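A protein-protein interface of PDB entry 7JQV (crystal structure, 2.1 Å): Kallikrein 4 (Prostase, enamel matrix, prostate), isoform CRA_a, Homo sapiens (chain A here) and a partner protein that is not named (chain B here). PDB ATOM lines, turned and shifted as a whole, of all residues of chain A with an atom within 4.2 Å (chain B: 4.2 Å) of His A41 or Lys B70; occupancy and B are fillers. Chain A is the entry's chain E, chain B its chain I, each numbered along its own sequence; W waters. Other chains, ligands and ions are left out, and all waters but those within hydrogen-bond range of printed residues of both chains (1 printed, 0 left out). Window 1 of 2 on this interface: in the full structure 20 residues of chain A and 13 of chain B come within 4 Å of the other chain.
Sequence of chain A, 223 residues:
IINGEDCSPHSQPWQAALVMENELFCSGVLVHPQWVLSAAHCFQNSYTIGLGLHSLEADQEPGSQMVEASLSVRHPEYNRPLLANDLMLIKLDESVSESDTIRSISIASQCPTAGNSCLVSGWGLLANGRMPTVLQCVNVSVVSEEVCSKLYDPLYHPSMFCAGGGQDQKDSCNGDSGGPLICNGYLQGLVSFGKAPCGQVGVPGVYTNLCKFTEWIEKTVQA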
ATOM      1  N   ALA A  39     -23.087  -8.173  -9.390  1.00  0.00           N
ATOM      2  CA  ALA A  39     -24.040  -7.259  -9.994  1.00  0.00           C
ATOM      3  C   ALA A  39     -23.963  -7.404 -11.514  1.00  0.00           C
ATOM      4  O   ALA A  39     -22.861  -7.452 -12.092  1.00  0.00           O
ATOM      5  CB  ALA A  39     -23.758  -5.830  -9.557  1.00  0.00           C
ATOM      6  N   ALA A  40     -25.152  -7.418 -12.174  1.00  0.00           N
ATOM      7  CA  ALA A  40     -25.202  -7.422 -13.632  1.00  0.00           C
ATOM      8  C   ALA A  40     -24.405  -6.217 -14.167  1.00  0.00           C
ATOM      9  O   ALA A  40     -23.869  -6.274 -15.244  1.00  0.00           O
ATOM     10  CB  ALA A  40     -26.674  -7.468 -14.161  1.00  0.00           C
ATOM     11  N   HIS A  41     -24.365  -5.074 -13.459  1.00  0.00           N
ATOM     12  CA  HIS A  41     -23.641  -3.922 -14.033  1.00  0.00           C
ATOM     13  C   HIS A  41     -22.130  -4.120 -14.122  1.00  0.00           C
ATOM     14  O   HIS A  41     -21.406  -3.342 -14.792  1.00  0.00           O
ATOM     15  CB  HIS A  41     -24.130  -2.621 -13.303  1.00  0.00           C
ATOM     16  CG  HIS A  41     -23.516  -2.476 -11.940  1.00  0.00           C
ATOM     17  ND1 HIS A  41     -24.258  -2.647 -10.764  1.00  0.00           N
ATOM     18  CD2 HIS A  41     -22.317  -1.945 -11.573  1.00  0.00           C
ATOM     19  CE1 HIS A  41     -23.525  -2.299  -9.697  1.00  0.00           C
ATOM     20  NE2 HIS A  41     -22.299  -1.872 -10.173  1.00  0.00           N
ATOM     21  N   CYS A  42     -21.614  -5.184 -13.451  1.00  0.00           N
ATOM     22  CA  CYS A  42     -20.191  -5.463 -13.519  1.00  0.00           C
ATOM     23  C   CYS A  42     -19.856  -6.378 -14.723  1.00  0.00           C
ATOM     24  O   CYS A  42     -18.707  -6.854 -14.853  1.00  0.00           O
ATOM     25  CB  CYS A  42     -19.721  -6.186 -12.236  1.00  0.00           C
ATOM     26  SG  CYS A  42     -20.008  -5.106 -10.767  1.00  0.00           S
ATOM     27  N   PHE A  43     -20.849  -6.704 -15.559  1.00  0.00           N
ATOM     28  CA  PHE A  43     -20.621  -7.652 -16.675  1.00  0.00           C
ATOM     29  C   PHE A  43     -19.404  -7.267 -17.505  1.00  0.00           C
ATOM     30  O   PHE A  43     -19.220  -6.093 -17.836  1.00  0.00           O
ATOM     31  CB  PHE A  43     -21.814  -7.660 -17.667  1.00  0.00           C
ATOM     32  CG  PHE A  43     -21.615  -8.566 -18.866  1.00  0.00           C
ATOM     33  CD1 PHE A  43     -21.889  -9.941 -18.783  1.00  0.00           C
ATOM     34  CD2 PHE A  43     -21.166  -8.040 -20.066  1.00  0.00           C
ATOM     35  CE1 PHE A  43     -21.680 -10.776 -19.885  1.00  0.00           C
ATOM     36  CE2 PHE A  43     -20.949  -8.874 -21.161  1.00  0.00           C
ATOM     37  CZ  PHE A  43     -21.196 -10.228 -21.071  1.00  0.00           C
ATOM     38  N   GLN A  44     -18.609  -8.300 -17.826  1.00  0.00           N
ATOM     39  CA  GLN A  44     -17.566  -8.249 -18.823  1.00  0.00           C
ATOM     40  C   GLN A  44     -17.593  -9.564 -19.622  1.00  0.00           C
ATOM     41  O   GLN A  44     -18.095 -10.585 -19.131  1.00  0.00           O
ATOM     42  CB  GLN A  44     -16.179  -8.082 -18.139  1.00  0.00           C
ATOM     43  CG  GLN A  44     -16.015  -6.751 -17.396  1.00  0.00           C
ATOM     44  CD  GLN A  44     -15.780  -5.675 -18.445  1.00  0.00           C
ATOM     45  OE1 GLN A  44     -14.673  -5.491 -18.954  1.00  0.00           O
ATOM     46  NE2 GLN A  44     -16.817  -4.934 -18.796  1.00  0.00           N
ATOM     47  N   TYR A  78     -32.654  -7.628 -16.169  1.00  0.00           N
ATOM     48  CA  TYR A  78     -31.680  -6.584 -15.797  1.00  0.00           C
ATOM     49  C   TYR A  78     -32.005  -5.268 -16.480  1.00  0.00           C
ATOM     50  O   TYR A  78     -32.093  -5.226 -17.720  1.00  0.00           O
ATOM     51  CB  TYR A  78     -30.212  -7.005 -16.021  1.00  0.00           C
ATOM     52  CG  TYR A  78     -29.211  -5.874 -15.827  1.00  0.00           C
ATOM     53  CD1 TYR A  78     -29.172  -5.130 -14.640  1.00  0.00           C
ATOM     54  CD2 TYR A  78     -28.344  -5.479 -16.850  1.00  0.00           C
ATOM     55  CE1 TYR A  78     -28.250  -4.104 -14.462  1.00  0.00           C
ATOM     56  CE2 TYR A  78     -27.469  -4.396 -16.695  1.00  0.00           C
ATOM     57  CZ  TYR A  78     -27.363  -3.782 -15.473  1.00  0.00           C
ATOM     58  OH  TYR A  78     -26.549  -2.707 -15.316  1.00  0.00           O
ATOM     59  N   ASP A  86     -30.551  -6.365 -10.691  1.00  0.00           N
ATOM     60  CA  ASP A  86     -29.112  -6.202 -10.867  1.00  0.00           C
ATOM     61  C   ASP A  86     -28.348  -7.398 -10.286  1.00  0.00           C
ATOM     62  O   ASP A  86     -27.691  -7.265  -9.232  1.00  0.00           O
ATOM     63  CB  ASP A  86     -28.638  -4.891 -10.216  1.00  0.00           C
ATOM     64  CG  ASP A  86     -27.233  -4.438 -10.622  1.00  0.00           C
ATOM     65  OD1 ASP A  86     -26.561  -5.088 -11.507  1.00  0.00           O
ATOM     66  OD2 ASP A  86     -26.807  -3.387 -10.036  1.00  0.00           O
ATOM     67  N   SER A 177     -19.434  -2.507  -5.474  1.00  0.00           N
ATOM     68  CA  SER A 177     -20.480  -3.091  -6.301  1.00  0.00           C
ATOM     69  C   SER A 177     -20.285  -4.610  -6.413  1.00  0.00           C
ATOM     70  O   SER A 177     -19.183  -5.032  -6.629  1.00  0.00           O
ATOM     71  CB  SER A 177     -20.438  -2.504  -7.706  1.00  0.00           C
ATOM     72  OG  SER A 177     -21.219  -1.322  -7.796  1.00  0.00           O
ATOM     73  N   SER A 192     -25.267  -2.463  -4.922  1.00  0.00           N
ATOM     74  CA  SER A 192     -25.756  -2.154  -6.272  1.00  0.00           C
ATOM     75  C   SER A 192     -25.539  -0.666  -6.610  1.00  0.00           C
ATOM     76  O   SER A 192     -24.699  -0.337  -7.435  1.00  0.00           O
ATOM     77  CB  SER A 192     -27.264  -2.554  -6.441  1.00  0.00           C
ATOM     78  OG  SER A 192     -27.679  -2.319  -7.820  1.00  0.00           O
ATOM     79  N   GLY B   1     -21.196  -1.387 -25.991  1.00  0.00           N
ATOM     80  CA  GLY B   1     -21.916  -1.341 -24.716  1.00  0.00           C
ATOM     81  C   GLY B   1     -21.054  -1.730 -23.493  1.00  0.00           C
ATOM     82  O   GLY B   1     -20.806  -0.885 -22.602  1.00  0.00           O
ATOM     83  N   SER B   2     -20.633  -3.010 -23.386  1.00  0.00           N
ATOM     84  CA  SER B   2     -19.907  -3.497 -22.199  1.00  0.00           C
ATOM     85  C   SER B   2     -18.443  -3.027 -22.198  1.00  0.00           C
ATOM     86  O   SER B   2     -17.610  -3.369 -21.316  1.00  0.00           O
ATOM     87  CB  SER B   2     -20.010  -4.995 -22.012  1.00  0.00           C
ATOM     88  OG  SER B   2     -18.916  -5.670 -22.651  1.00  0.00           O
ATOM     89  N   SER B   3     -18.160  -2.187 -23.190  1.00  0.00           N
ATOM     90  CA  SER B   3     -16.863  -1.568 -23.323  1.00  0.00           C
ATOM     91  C   SER B   3     -16.739  -0.544 -22.207  1.00  0.00           C
ATOM     92  O   SER B   3     -17.677   0.198 -21.964  1.00  0.00           O
ATOM     93  CB  SER B   3     -16.752  -0.913 -24.654  1.00  0.00           C
ATOM     94  OG  SER B   3     -16.336  -1.867 -25.625  1.00  0.00           O
ATOM     95  N   VAL B   5     -15.057   2.817 -20.818  1.00  0.00           N
ATOM     96  CA  VAL B   5     -14.506   4.060 -21.321  1.00  0.00           C
ATOM     97  C   VAL B   5     -13.082   4.260 -20.771  1.00  0.00           C
ATOM     98  O   VAL B   5     -12.866   4.164 -19.543  1.00  0.00           O
ATOM     99  CB  VAL B   5     -15.445   5.222 -20.930  1.00  0.00           C
ATOM    100  CG1 VAL B   5     -14.877   6.567 -21.453  1.00  0.00           C
ATOM    101  CG2 VAL B   5     -16.823   4.984 -21.594  1.00  0.00           C
ATOM    102  N   LEU B  64     -24.223   3.757  -9.716  1.00  0.00           N
ATOM    103  CA  LEU B  64     -23.669   2.427  -9.483  1.00  0.00           C
ATOM    104  C   LEU B  64     -22.446   2.493  -8.559  1.00  0.00           C
ATOM    105  O   LEU B  64     -21.569   3.357  -8.674  1.00  0.00           O
ATOM    106  CB  LEU B  64     -23.342   1.757 -10.839  1.00  0.00           C
ATOM    107  CG  LEU B  64     -24.539   1.601 -11.832  1.00  0.00           C
ATOM    108  CD1 LEU B  64     -24.021   1.172 -13.182  1.00  0.00           C
ATOM    109  CD2 LEU B  64     -25.586   0.568 -11.332  1.00  0.00           C
ATOM    110  N   ILE B  66     -19.633   1.250  -8.639  1.00  0.00           N
ATOM    111  CA  ILE B  66     -18.464   0.792  -9.381  1.00  0.00           C
ATOM    112  C   ILE B  66     -17.575   2.036  -9.630  1.00  0.00           C
ATOM    113  O   ILE B  66     -18.082   3.177  -9.602  1.00  0.00           O
ATOM    114  CB  ILE B  66     -18.967   0.050 -10.670  1.00  0.00           C
ATOM    115  CG1 ILE B  66     -17.854  -0.718 -11.386  1.00  0.00           C
ATOM    116  CG2 ILE B  66     -19.649   1.042 -11.621  1.00  0.00           C
ATOM    117  CD1 ILE B  66     -18.305  -1.594 -12.602  1.00  0.00           C
ATOM    118  N   ILE B  69     -16.475   3.395 -15.766  1.00  0.00           N
ATOM    119  CA  ILE B  69     -17.670   3.834 -16.514  1.00  0.00           C
ATOM    120  C   ILE B  69     -17.732   2.941 -17.758  1.00  0.00           C
ATOM    121  O   ILE B  69     -16.738   2.886 -18.473  1.00  0.00           O
ATOM    122  CB  ILE B  69     -17.451   5.323 -16.934  1.00  0.00           C
ATOM    123  CG1 ILE B  69     -17.479   6.260 -15.726  1.00  0.00           C
ATOM    124  CG2 ILE B  69     -18.472   5.755 -17.984  1.00  0.00           C
ATOM    125  CD1 ILE B  69     -18.656   6.002 -14.827  1.00  0.00           C
ATOM    126  N   LYS B  70     -18.904   2.375 -18.101  1.00  0.00           N
ATOM    127  CA  LYS B  70     -19.044   1.702 -19.378  1.00  0.00           C
ATOM    128  C   LYS B  70     -19.856   2.576 -20.301  1.00  0.00           C
ATOM    129  O   LYS B  70     -20.596   3.478 -19.897  1.00  0.00           O
ATOM    130  CB  LYS B  70     -19.815   0.365 -19.217  1.00  0.00           C
ATOM    131  CG  LYS B  70     -19.008  -0.700 -18.437  1.00  0.00           C
ATOM    132  CD  LYS B  70     -20.048  -1.860 -18.406  1.00  0.00           C
ATOM    133  CE  LYS B  70     -19.802  -2.956 -17.481  1.00  0.00           C
ATOM    134  NZ  LYS B  70     -20.912  -3.892 -17.775  1.00  0.00           N
ATOM    135  N   GLU B  71     -19.752   2.266 -21.586  1.00  0.00           N
ATOM    136  CA  GLU B  71     -20.405   3.091 -22.591  1.00  0.00           C
ATOM    137  C   GLU B  71     -21.905   2.928 -22.474  1.00  0.00           C
ATOM    138  O   GLU B  71     -22.644   3.768 -22.971  1.00  0.00           O
ATOM    139  CB  GLU B  71     -19.994   2.594 -24.001  1.00  0.00           C
ATOM    140  CG  GLU B  71     -18.523   2.843 -24.261  1.00  0.00           C
ATOM    141  CD  GLU B  71     -18.077   2.516 -25.703  1.00  0.00           C
ATOM    142  OE1 GLU B  71     -18.873   2.710 -26.650  1.00  0.00           O
ATOM    143  OE2 GLU B  71     -16.911   2.115 -25.883  1.00  0.00           O
ATOM    144  N   SER B  72     -22.369   1.824 -21.880  1.00  0.00           N
ATOM    145  CA  SER B  72     -23.823   1.640 -21.801  1.00  0.00           C
ATOM    146  C   SER B  72     -24.424   2.376 -20.585  1.00  0.00           C
ATOM    147  O   SER B  72     -25.644   2.388 -20.401  1.00  0.00           O
ATOM    148  CB  SER B  72     -24.154   0.128 -21.739  1.00  0.00           C
ATOM    149  OG  SER B  72     -23.618  -0.354 -20.495  1.00  0.00           O
ATOM    150  N   TYR B  73     -23.586   2.938 -19.696  1.00  0.00           N
ATOM    151  CA  TYR B  73     -24.162   3.531 -18.489  1.00  0.00           C
ATOM    152  C   TYR B  73     -24.851   4.875 -18.775  1.00  0.00           C
ATOM    153  O   TYR B  73     -24.307   5.689 -19.501  1.00  0.00           O
ATOM    154  CB  TYR B  73     -23.087   3.817 -17.427  1.00  0.00           C
ATOM    155  CG  TYR B  73     -22.508   2.607 -16.712  1.00  0.00           C
ATOM    156  CD1 TYR B  73     -23.054   1.295 -16.862  1.00  0.00           C
ATOM    157  CD2 TYR B  73     -21.410   2.747 -15.861  1.00  0.00           C
ATOM    158  CE1 TYR B  73     -22.458   0.191 -16.216  1.00  0.00           C
ATOM    159  CE2 TYR B  73     -20.789   1.633 -15.250  1.00  0.00           C
ATOM    160  CZ  TYR B  73     -21.335   0.351 -15.412  1.00  0.00           C
ATOM    161  OH  TYR B  73     -20.762  -0.734 -14.759  1.00  0.00           O
HETATM  162  O   HOH W   1     -23.694  -4.794 -17.760  1.00  0.00           O
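Of chain B, only Leu B64, Ile B66, Lys B70 and Tyr B73 come within 4 Å of His A41.
Lys B70 touches just these residues of chain A: His A41 (3.1 Å), Phe A43 (2.8 Å) and Gln A44 (3.8 Å).
Of the printed residues of chain B, Phe A43 touches Ser B2 and Lys B70.
Of the printed residues of chain A, Leu B64 touches His A41 (3.5 Å) and Ser A192 (3.6 Å).
Of the printed residues of chain B, Ser A177 touches Ile B66.
Printed residues of chain B within 4 Å of Ser A192: Leu B64.
Of the printed residues of chain A, Ile B66 touches His A41 (3.9 Å) and Ser A177 (3.1 Å).
The nearest printed residue of chain B that does not touch His A41 is Ser B72 (6.8 Å).
The side-chain carboxylate of Asp A86 sits at hydrogen-bond distance from the side-chain hydroxyl of Ser A192 (2.6 Å).
A ring nitrogen (NE2) of His A41 lies within hydrogen-bond range of the side-chain hydroxyl (OG) of Ser A177 (2.7 Å).
A ring nitrogen (ND1) of His A41 is in hydrogen-bond range of the side-chain carboxylate (OD2) of Asp A86 (2.8 Å).
The backbone carbonyl oxygen (O) of His A41 lies within hydrogen-bond range of the side-chain amino group (NZ) of Lys B70 (3.1 Å).
The side-chain amide nitrogen of Gln A44 sits at hydrogen-bond distance from the backbone carbonyl oxygen of Ser B2.
The side-chain hydroxyl (OG) of Ser A177 sits at hydrogen-bond distance from the backbone NH (N) of Ile B66 (3.1 Å).
OH of Tyr B73 lies within hydrogen-bond range of O of His A41, 2.7 Å away.
O of Phe A43 sits at hydrogen-bond distance from NZ of Lys B70, 2.8 Å away.
Of the 10 printed residues of chain A, 5 touch a printed residue of chain B.
Hydrophobic or aromatic side chains of chain B within 4 Å of the printed part of chain A: Leu B64, Ile B66 and Tyr B73.
Among the printed residues, 10 pairs touch across the chains.
Among the printed residues, no Asp or Glu carboxylate lies within 4 Å of a Lys or Arg side-chain nitrogen of the other chain.
Water W1 lies within hydrogen-bond range of NZ of Lys B70 (2.9 Å) and O of Ala A40 (2.9 Å).
Among the printed residues, merely in contact across the chains: His A41 with Leu B64 (3.5 Å), His A41 with Ile B66 (3.9 Å), Phe A43 with Ser B2 (3.8 Å), Gln A44 with Lys B70 (3.8 Å) and Ser A192 with Leu B64 (3.6 Å).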
